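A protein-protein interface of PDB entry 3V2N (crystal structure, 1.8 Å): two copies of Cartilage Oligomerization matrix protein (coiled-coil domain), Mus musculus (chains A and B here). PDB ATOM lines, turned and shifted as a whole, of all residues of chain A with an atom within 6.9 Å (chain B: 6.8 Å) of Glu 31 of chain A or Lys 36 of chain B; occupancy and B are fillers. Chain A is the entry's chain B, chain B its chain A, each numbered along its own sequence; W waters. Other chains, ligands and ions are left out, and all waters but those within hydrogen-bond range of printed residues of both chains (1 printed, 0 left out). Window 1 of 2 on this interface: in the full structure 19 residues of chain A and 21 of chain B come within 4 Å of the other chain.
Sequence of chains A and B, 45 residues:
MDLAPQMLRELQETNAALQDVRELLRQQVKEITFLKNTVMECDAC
Glu 31 of chain A touches just these residues of chain B: Ile 32, Thr 33 and Lys 36.
Of the printed residues of chain B, Phe 34 of chain A touches Lys 36 and Met 40.
Printed residues of chain B within 4 Å of Leu 35 of chain A: Leu 35 (3.8 Å) and Val 39 (3.5 Å).
Printed residues of chain A within 4 Å of Ile 32 of chain B: Gln 28 (3.2 Å) and Glu 31 (3.9 Å).
Printed residues of chain A within 4 Å of Lys 36 of chain B: Glu 31 (2.7 Å) and Phe 34 (3.7 Å).
Printed residues of chain A within 4 Å of Met 40 of chain B: Phe 34 (3.8 Å).
Glu 41 of chain B touches none of the printed residues of chain A.
The nearest residue of chain B that does not touch Glu 31 of chain A is Val 29 of chain B (5.0 Å).
The nearest residue of chain A that does not touch Lys 36 of chain B is Leu 35 of chain A (4.04 Å).
The nearest printed residue of chain A that does not touch Val 29 of chain B is Glu 31 of chain A (5.0 Å).
Water W1 bridges the side-chain amino group (NZ) of Lys 36 of chain B (3.3 Å) and the side-chain carboxylate (OE1) of Glu 31 of chain A (3.4 Å).
Gln 27 of chain A touches Val 29 of chain B.
OE1 of Gln 28 of chain A touches CG2 of Val 29 of chain B, at 3.7 Å.
Ile 32 of chain B touches Gln 28 of chain A (CD1 to OE1, 3.2 Å).
CG2 of Ile 32 of chain B touches CB of Glu 31 of chain A, 3.9 Å away.
Phe 34 of chain A touches Lys 36 of chain B.
Phe 34 of chain A touches Met 40 of chain B.
Leu 35 of chain B touches Leu 35 of chain A (CD2 to CD2, 3.8 Å).
Leu 35 of chain A touches Val 39 of chain B (CD1 to CG2, 3.5 Å).
Val 39 of chain B touches Thr 38 of chain A (CG1 to CG2, 3.9 Å).
Glu 31 of chain A touches Ile 32 of chain B, but with the chains exchanged Ile 32 of chain A does not touch Glu 31 of chain B (8.7 Å).
Glu 31 of chain A touches Lys 36 of chain B, but with the chains exchanged Lys 36 of chain A does not touch Glu 31 of chain B (12.2 Å).
Phe 34 of chain A touches Lys 36 of chain B, but with the chains exchanged Lys 36 of chain A does not touch Phe 34 of chain B (11.7 Å).
Leu 35 of chain A touches its own counterpart, Leu 35 of chain B.
Positions printed for both chains: 29, 31, 32, 33, 34, 35, 36 and 38.
Of the 11 pairs that touch across the chains among the printed residues, 1 has its exchanged pair printed and touching as well.
The backbone carbonyl oxygen (O) of Val 29 of chain B lies within hydrogen-bond range of the side-chain hydroxyl (OG1) of Thr 33 of chain B.
The side-chain amide nitrogen (ND2) of Asn 37 of chain B sits at hydrogen-bond distance from the backbone carbonyl oxygen (O) of Thr 33 of chain B (3.1 Å).
The backbone carbonyl oxygen of Phe 34 of chain A is in hydrogen-bond range of the side-chain hydroxyl of Thr 38 of chain A, at 2.7 Å.
OG1 of Thr 33 of chain B is in hydrogen-bond range of OE1 of Glu 31 of chain A (3.1 Å).
NZ of Lys 36 of chain B lies within salt-bridge range of OE1 of Glu 31 of chain A (2.7 Å).
Of the 12 printed residues of chain A, 6 touch a printed residue of chain B.
Printed residues of chain A that touch a printed residue of chain B: Gln 27, Gln 28, Glu 31, Phe 34, Leu 35 and Thr 38.
Hydrophobic or aromatic side chains of chain B that line the printed part of chain A: Val 29, Ile 32, Leu 35, Val 39 and Met 40.
Among the printed residues, Asp or Glu carboxylates within 4 Å of a Lys or Arg side-chain nitrogen of the other chain: Glu 31 of chain A with Lys 36 of chain B.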
ATOM      1  N   ARG A  26     -23.318   5.959  -7.611  1.00  0.00           N
ATOM      2  CA  ARG A  26     -22.808   7.319  -7.486  1.00  0.00           C
ATOM      3  C   ARG A  26     -21.958   7.664  -8.702  1.00  0.00           C
ATOM      4  O   ARG A  26     -22.142   8.716  -9.322  1.00  0.00           O
ATOM      5  CB  ARG A  26     -21.977   7.477  -6.208  1.00  0.00           C
ATOM      6  CG  ARG A  26     -22.796   7.453  -4.924  1.00  0.00           C
ATOM      7  CD  ARG A  26     -21.955   7.832  -3.712  1.00  0.00           C
ATOM      8  NE  ARG A  26     -22.753   7.871  -2.489  1.00  0.00           N
ATOM      9  CZ  ARG A  26     -23.803   8.665  -2.306  1.00  0.00           C
ATOM     10  NH1 ARG A  26     -24.185   9.493  -3.267  1.00  0.00           N
ATOM     11  NH2 ARG A  26     -24.478   8.630  -1.164  1.00  0.00           N
ATOM     12  N   GLN A  27     -21.029   6.778  -9.046  1.00  0.00           N
ATOM     13  CA  GLN A  27     -20.188   7.026 -10.206  1.00  0.00           C
ATOM     14  C   GLN A  27     -21.004   7.014 -11.490  1.00  0.00           C
ATOM     15  O   GLN A  27     -20.720   7.772 -12.411  1.00  0.00           O
ATOM     16  CB  GLN A  27     -19.038   6.014 -10.294  1.00  0.00           C
ATOM     17  CG  GLN A  27     -19.358   4.599  -9.871  1.00  0.00           C
ATOM     18  CD  GLN A  27     -18.118   3.703  -9.869  1.00  0.00           C
ATOM     19  OE1 GLN A  27     -17.629   3.295 -10.924  1.00  0.00           O
ATOM     20  NE2 GLN A  27     -17.600   3.408  -8.679  1.00  0.00           N
ATOM     21  N   GLN A  28     -22.035   6.176 -11.545  1.00  0.00           N
ATOM     22  CA  GLN A  28     -22.859   6.099 -12.747  1.00  0.00           C
ATOM     23  C   GLN A  28     -23.633   7.400 -12.965  1.00  0.00           C
ATOM     24  O   GLN A  28     -23.711   7.899 -14.080  1.00  0.00           O
ATOM     25  CB  GLN A  28     -23.830   4.909 -12.666  1.00  0.00           C
ATOM     26  CG  GLN A  28     -24.723   4.754 -13.898  1.00  0.00           C
ATOM     27  CD  GLN A  28     -25.467   3.422 -13.926  1.00  0.00           C
ATOM     28  OE1 GLN A  28     -24.967   2.412 -14.441  1.00  0.00           O
ATOM     29  NE2 GLN A  28     -26.663   3.412 -13.360  1.00  0.00           N
ATOM     30  N   VAL A  29     -24.185   7.961 -11.898  1.00  0.00           N
ATOM     31  CA  VAL A  29     -24.935   9.205 -12.033  1.00  0.00           C
ATOM     32  C   VAL A  29     -24.018  10.345 -12.502  1.00  0.00           C
ATOM     33  O   VAL A  29     -24.453  11.253 -13.209  1.00  0.00           O
ATOM     34  CB  VAL A  29     -25.615   9.590 -10.690  1.00  0.00           C
ATOM     35  CG1 VAL A  29     -26.316  10.930 -10.826  1.00  0.00           C
ATOM     36  CG2 VAL A  29     -26.611   8.514 -10.294  1.00  0.00           C
ATOM     37  N   LYS A  30     -22.746  10.286 -12.124  1.00  0.00           N
ATOM     38  CA  LYS A  30     -21.788  11.318 -12.515  1.00  0.00           C
ATOM     39  C   LYS A  30     -21.489  11.231 -14.015  1.00  0.00           C
ATOM     40  O   LYS A  30     -21.367  12.249 -14.690  1.00  0.00           O
ATOM     41  CB  LYS A  30     -20.493  11.175 -11.704  1.00  0.00           C
ATOM     42  CG  LYS A  30     -19.507  12.323 -11.918  1.00  0.00           C
ATOM     43  CD  LYS A  30     -18.307  12.214 -10.992  1.00  0.00           C
ATOM     44  CE  LYS A  30     -17.394  13.432 -11.141  1.00  0.00           C
ATOM     45  NZ  LYS A  30     -16.213  13.356 -10.236  1.00  0.00           N
ATOM     46  N   GLU A  31     -21.368  10.009 -14.526  1.00  0.00           N
ATOM     47  CA  GLU A  31     -21.101   9.788 -15.947  1.00  0.00           C
ATOM     48  C   GLU A  31     -22.305  10.238 -16.778  1.00  0.00           C
ATOM     49  O   GLU A  31     -22.157  10.867 -17.825  1.00  0.00           O
ATOM     50  CB  GLU A  31     -20.835   8.306 -16.203  1.00  0.00           C
ATOM     51  CG  GLU A  31     -19.610   7.747 -15.493  1.00  0.00           C
ATOM     52  CD  GLU A  31     -18.324   8.382 -15.978  1.00  0.00           C
ATOM     53  OE1 GLU A  31     -17.925   8.121 -17.131  1.00  0.00           O
ATOM     54  OE2 GLU A  31     -17.717   9.151 -15.207  1.00  0.00           O
ATOM     55  N   ILE A  32     -23.503   9.905 -16.309  1.00  0.00           N
ATOM     56  CA  ILE A  32     -24.717  10.273 -17.024  1.00  0.00           C
ATOM     57  C   ILE A  32     -24.898  11.782 -17.045  1.00  0.00           C
ATOM     58  O   ILE A  32     -25.324  12.344 -18.053  1.00  0.00           O
ATOM     59  CB  ILE A  32     -25.973   9.622 -16.383  1.00  0.00           C
ATOM     60  CG1 ILE A  32     -25.960   8.110 -16.638  1.00  0.00           C
ATOM     61  CG2 ILE A  32     -27.245  10.266 -16.957  1.00  0.00           C
ATOM     62  CD1 ILE A  32     -27.061   7.346 -15.920  1.00  0.00           C
ATOM     63  N   THR A  33     -24.584  12.435 -15.929  1.00  0.00           N
ATOM     64  CA  THR A  33     -24.706  13.885 -15.842  1.00  0.00           C
ATOM     65  C   THR A  33     -23.746  14.528 -16.849  1.00  0.00           C
ATOM     66  O   THR A  33     -24.097  15.496 -17.520  1.00  0.00           O
ATOM     67  CB  THR A  33     -24.396  14.388 -14.404  1.00  0.00           C
ATOM     68  OG1 THR A  33     -25.288  13.754 -13.471  1.00  0.00           O
ATOM     69  CG2 THR A  33     -24.576  15.901 -14.316  1.00  0.00           C
ATOM     70  N   PHE A  34     -22.543  13.970 -16.962  1.00  0.00           N
ATOM     71  CA  PHE A  34     -21.541  14.482 -17.896  1.00  0.00           C
ATOM     72  C   PHE A  34     -21.990  14.248 -19.341  1.00  0.00           C
ATOM     73  O   PHE A  34     -21.722  15.062 -20.222  1.00  0.00           O
ATOM     74  CB  PHE A  34     -20.192  13.797 -17.667  1.00  0.00           C
ATOM     75  CG  PHE A  34     -19.021  14.586 -18.190  1.00  0.00           C
ATOM     76  CD1 PHE A  34     -18.362  15.500 -17.375  1.00  0.00           C
ATOM     77  CD2 PHE A  34     -18.601  14.441 -19.510  1.00  0.00           C
ATOM     78  CE1 PHE A  34     -17.302  16.266 -17.871  1.00  0.00           C
ATOM     79  CE2 PHE A  34     -17.545  15.200 -20.016  1.00  0.00           C
ATOM     80  CZ  PHE A  34     -16.893  16.114 -19.194  1.00  0.00           C
ATOM     81  N   LEU A  35     -22.662  13.127 -19.576  1.00  0.00           N
ATOM     82  CA  LEU A  35     -23.168  12.805 -20.909  1.00  0.00           C
ATOM     83  C   LEU A  35     -24.281  13.802 -21.255  1.00  0.00           C
ATOM     84  O   LEU A  35     -24.342  14.297 -22.372  1.00  0.00           O
ATOM     85  CB  LEU A  35     -23.713  11.370 -20.941  1.00  0.00           C
ATOM     86  CG  LEU A  35     -24.400  10.896 -22.230  1.00  0.00           C
ATOM     87  CD1 LEU A  35     -23.426  10.983 -23.405  1.00  0.00           C
ATOM     88  CD2 LEU A  35     -24.893   9.465 -22.047  1.00  0.00           C
ATOM     89  N   LYS A  36     -25.150  14.096 -20.288  1.00  0.00           N
ATOM     90  CA  LYS A  36     -26.247  15.046 -20.506  1.00  0.00           C
ATOM     91  C   LYS A  36     -25.706  16.397 -20.968  1.00  0.00           C
ATOM     92  O   LYS A  36     -26.114  16.925 -22.006  1.00  0.00           O
ATOM     93  CB  LYS A  36     -27.044  15.266 -19.212  1.00  0.00           C
ATOM     94  CG  LYS A  36     -28.118  16.349 -19.333  1.00  0.00           C
ATOM     95  CD  LYS A  36     -28.661  16.790 -17.976  1.00  0.00           C
ATOM     96  CE  LYS A  36     -27.607  17.562 -17.173  1.00  0.00           C
ATOM     97  NZ  LYS A  36     -28.099  17.983 -15.819  1.00  0.00           N
ATOM     98  N   THR A  38     -22.805  17.184 -22.178  1.00  0.00           N
ATOM     99  CA  THR A  38     -22.058  17.115 -23.427  1.00  0.00           C
ATOM    100  C   THR A  38     -22.994  17.160 -24.632  1.00  0.00           C
ATOM    101  O   THR A  38     -22.653  17.729 -25.672  1.00  0.00           O
ATOM    102  CB  THR A  38     -21.200  15.833 -23.500  1.00  0.00           C
ATOM    103  OG1 THR A  38     -20.267  15.814 -22.407  1.00  0.00           O
ATOM    104  CG2 THR A  38     -20.438  15.779 -24.820  1.00  0.00           C
ATOM    105  N   VAL B  29     -22.062   0.507 -15.700  1.00  0.00           N
ATOM    106  CA  VAL B  29     -21.262   1.714 -15.566  1.00  0.00           C
ATOM    107  C   VAL B  29     -20.212   1.730 -16.681  1.00  0.00           C
ATOM    108  O   VAL B  29     -19.995   2.754 -17.325  1.00  0.00           O
ATOM    109  CB  VAL B  29     -20.560   1.776 -14.189  1.00  0.00           C
ATOM    110  CG1 VAL B  29     -19.536   2.899 -14.171  1.00  0.00           C
ATOM    111  CG2 VAL B  29     -21.592   1.999 -13.098  1.00  0.00           C
ATOM    112  N   GLU B  31     -20.334   0.358 -19.619  1.00  0.00           N
ATOM    113  CA  GLU B  31     -21.006   0.645 -20.883  1.00  0.00           C
ATOM    114  C   GLU B  31     -21.359   2.133 -20.995  1.00  0.00           C
ATOM    115  O   GLU B  31     -21.178   2.745 -22.046  1.00  0.00           O
ATOM    116  CB  GLU B  31     -22.285  -0.185 -20.999  1.00  0.00           C
ATOM    117  CG  GLU B  31     -22.094  -1.692 -21.010  1.00  0.00           C
ATOM    118  CD  GLU B  31     -21.294  -2.193 -22.202  1.00  0.00           C
ATOM    119  OE1 GLU B  31     -21.411  -1.611 -23.296  1.00  0.00           O
ATOM    120  OE2 GLU B  31     -20.558  -3.187 -22.045  1.00  0.00           O
ATOM    121  N   ILE B  32     -21.860   2.710 -19.907  1.00  0.00           N
ATOM    122  CA  ILE B  32     -22.237   4.120 -19.892  1.00  0.00           C
ATOM    123  C   ILE B  32     -21.012   5.022 -20.047  1.00  0.00           C
ATOM    124  O   ILE B  32     -21.087   6.067 -20.683  1.00  0.00           O
ATOM    125  CB  ILE B  32     -22.970   4.478 -18.579  1.00  0.00           C
ATOM    126  CG1 ILE B  32     -24.356   3.826 -18.569  1.00  0.00           C
ATOM    127  CG2 ILE B  32     -23.040   5.993 -18.412  1.00  0.00           C
ATOM    128  CD1 ILE B  32     -25.043   3.869 -17.234  1.00  0.00           C
ATOM    129  N   THR B  33     -19.886   4.616 -19.469  1.00  0.00           N
ATOM    130  CA  THR B  33     -18.659   5.406 -19.571  1.00  0.00           C
ATOM    131  C   THR B  33     -18.151   5.341 -21.012  1.00  0.00           C
ATOM    132  O   THR B  33     -17.600   6.306 -21.546  1.00  0.00           O
ATOM    133  CB  THR B  33     -17.557   4.868 -18.623  1.00  0.00           C
ATOM    134  OG1 THR B  33     -17.985   5.002 -17.256  1.00  0.00           O
ATOM    135  CG2 THR B  33     -16.263   5.650 -18.812  1.00  0.00           C
ATOM    136  N   PHE B  34     -18.332   4.191 -21.645  1.00  0.00           N
ATOM    137  CA  PHE B  34     -17.895   4.042 -23.020  1.00  0.00           C
ATOM    138  C   PHE B  34     -18.771   4.938 -23.895  1.00  0.00           C
ATOM    139  O   PHE B  34     -18.273   5.651 -24.768  1.00  0.00           O
ATOM    140  CB  PHE B  34     -17.996   2.578 -23.457  1.00  0.00           C
ATOM    141  CG  PHE B  34     -17.248   2.282 -24.724  1.00  0.00           C
ATOM    142  CD1 PHE B  34     -17.773   2.645 -25.962  1.00  0.00           C
ATOM    143  CD2 PHE B  34     -15.989   1.694 -24.678  1.00  0.00           C
ATOM    144  CE1 PHE B  34     -17.055   2.432 -27.141  1.00  0.00           C
ATOM    145  CE2 PHE B  34     -15.258   1.475 -25.853  1.00  0.00           C
ATOM    146  CZ  PHE B  34     -15.795   1.847 -27.083  1.00  0.00           C
ATOM    147  N   LEU B  35     -20.071   4.919 -23.630  1.00  0.00           N
ATOM    148  CA  LEU B  35     -21.029   5.736 -24.373  1.00  0.00           C
ATOM    149  C   LEU B  35     -20.676   7.213 -24.228  1.00  0.00           C
ATOM    150  O   LEU B  35     -20.716   7.968 -25.198  1.00  0.00           O
ATOM    151  CB  LEU B  35     -22.447   5.489 -23.853  1.00  0.00           C
ATOM    152  CG  LEU B  35     -23.572   6.345 -24.455  1.00  0.00           C
ATOM    153  CD1 LEU B  35     -23.700   6.082 -25.958  1.00  0.00           C
ATOM    154  CD2 LEU B  35     -24.881   6.027 -23.755  1.00  0.00           C
ATOM    155  N   LYS B  36     -20.330   7.624 -23.011  1.00  0.00           N
ATOM    156  CA  LYS B  36     -19.960   9.012 -22.759  1.00  0.00           C
ATOM    157  C   LYS B  36     -18.747   9.403 -23.612  1.00  0.00           C
ATOM    158  O   LYS B  36     -18.790  10.387 -24.350  1.00  0.00           O
ATOM    159  CB  LYS B  36     -19.628   9.220 -21.276  1.00  0.00           C
ATOM    160  CG  LYS B  36     -19.166  10.640 -20.944  1.00  0.00           C
ATOM    161  CD  LYS B  36     -18.547  10.756 -19.558  1.00  0.00           C
ATOM    162  CE  LYS B  36     -17.216  10.018 -19.484  1.00  0.00           C
ATOM    163  NZ  LYS B  36     -16.556  10.156 -18.158  1.00  0.00           N
ATOM    164  N   ASN B  37     -17.675   8.623 -23.506  1.00  0.00           N
ATOM    165  CA  ASN B  37     -16.448   8.897 -24.250  1.00  0.00           C
ATOM    166  C   ASN B  37     -16.672   8.954 -25.756  1.00  0.00           C
ATOM    167  O   ASN B  37     -16.035   9.745 -26.455  1.00  0.00           O
ATOM    168  CB  ASN B  37     -15.379   7.842 -23.936  1.00  0.00           C
ATOM    169  CG  ASN B  37     -14.942   7.870 -22.487  1.00  0.00           C
ATOM    170  OD1 ASN B  37     -14.959   8.919 -21.845  1.00  0.00           O
ATOM    171  ND2 ASN B  37     -14.527   6.720 -21.967  1.00  0.00           N
ATOM    172  N   THR B  38     -17.570   8.109 -26.249  1.00  0.00           N
ATOM    173  CA  THR B  38     -17.888   8.057 -27.673  1.00  0.00           C
ATOM    174  C   THR B  38     -18.571   9.361 -28.089  1.00  0.00           C
ATOM    175  O   THR B  38     -18.253   9.935 -29.132  1.00  0.00           O
ATOM    176  CB  THR B  38     -18.822   6.859 -27.983  1.00  0.00           C
ATOM    177  OG1 THR B  38     -18.145   5.638 -27.647  1.00  0.00           O
ATOM    178  CG2 THR B  38     -19.200   6.837 -29.453  1.00  0.00           C
ATOM    179  N   VAL B  39     -19.495   9.831 -27.257  1.00  0.00           N
ATOM    180  CA  VAL B  39     -20.206  11.076 -27.542  1.00  0.00           C
ATOM    181  C   VAL B  39     -19.232  12.259 -27.531  1.00  0.00           C
ATOM    182  O   VAL B  39     -19.306  13.142 -28.392  1.00  0.00           O
ATOM    183  CB  VAL B  39     -21.334  11.301 -26.508  1.00  0.00           C
ATOM    184  CG1 VAL B  39     -21.937  12.689 -26.667  1.00  0.00           C
ATOM    185  CG2 VAL B  39     -22.408  10.242 -26.702  1.00  0.00           C
ATOM    186  N   MET B  40     -18.312  12.256 -26.566  1.00  0.00           N
ATOM    187  CA  MET B  40     -17.315  13.312 -26.431  1.00  0.00           C
ATOM    188  C   MET B  40     -16.444  13.427 -27.684  1.00  0.00           C
ATOM    189  O   MET B  40     -15.912  14.500 -27.983  1.00  0.00           O
ATOM    190  CB  MET B  40     -16.429  13.051 -25.205  1.00  0.00           C
ATOM    191  CG  MET B  40     -17.158  13.154 -23.853  1.00  0.00           C
ATOM    192  SD  MET B  40     -16.114  12.676 -22.454  1.00  0.00           S
ATOM    193  CE  MET B  40     -14.843  13.950 -22.564  1.00  0.00           C
ATOM    194  N   GLU B  41     -16.306  12.325 -28.414  1.00  0.00           N
ATOM    195  CA  GLU B  41     -15.502  12.313 -29.635  1.00  0.00           C
ATOM    196  C   GLU B  41     -16.343  12.412 -30.901  1.00  0.00           C
ATOM    197  O   GLU B  41     -15.824  12.255 -32.007  1.00  0.00           O
ATOM    198  CB  GLU B  41     -14.649  11.044 -29.715  1.00  0.00           C
ATOM    199  CG  GLU B  41     -13.166  11.263 -29.453  1.00  0.00           C
ATOM    200  CD  GLU B  41     -12.842  11.362 -27.983  1.00  0.00           C
ATOM    201  OE1 GLU B  41     -13.161  10.404 -27.248  1.00  0.00           O
ATOM    202  OE2 GLU B  41     -12.264  12.388 -27.565  1.00  0.00           O
HETATM  203  O   HOH W   1     -14.506   7.781 -17.168  1.00  0.00           O
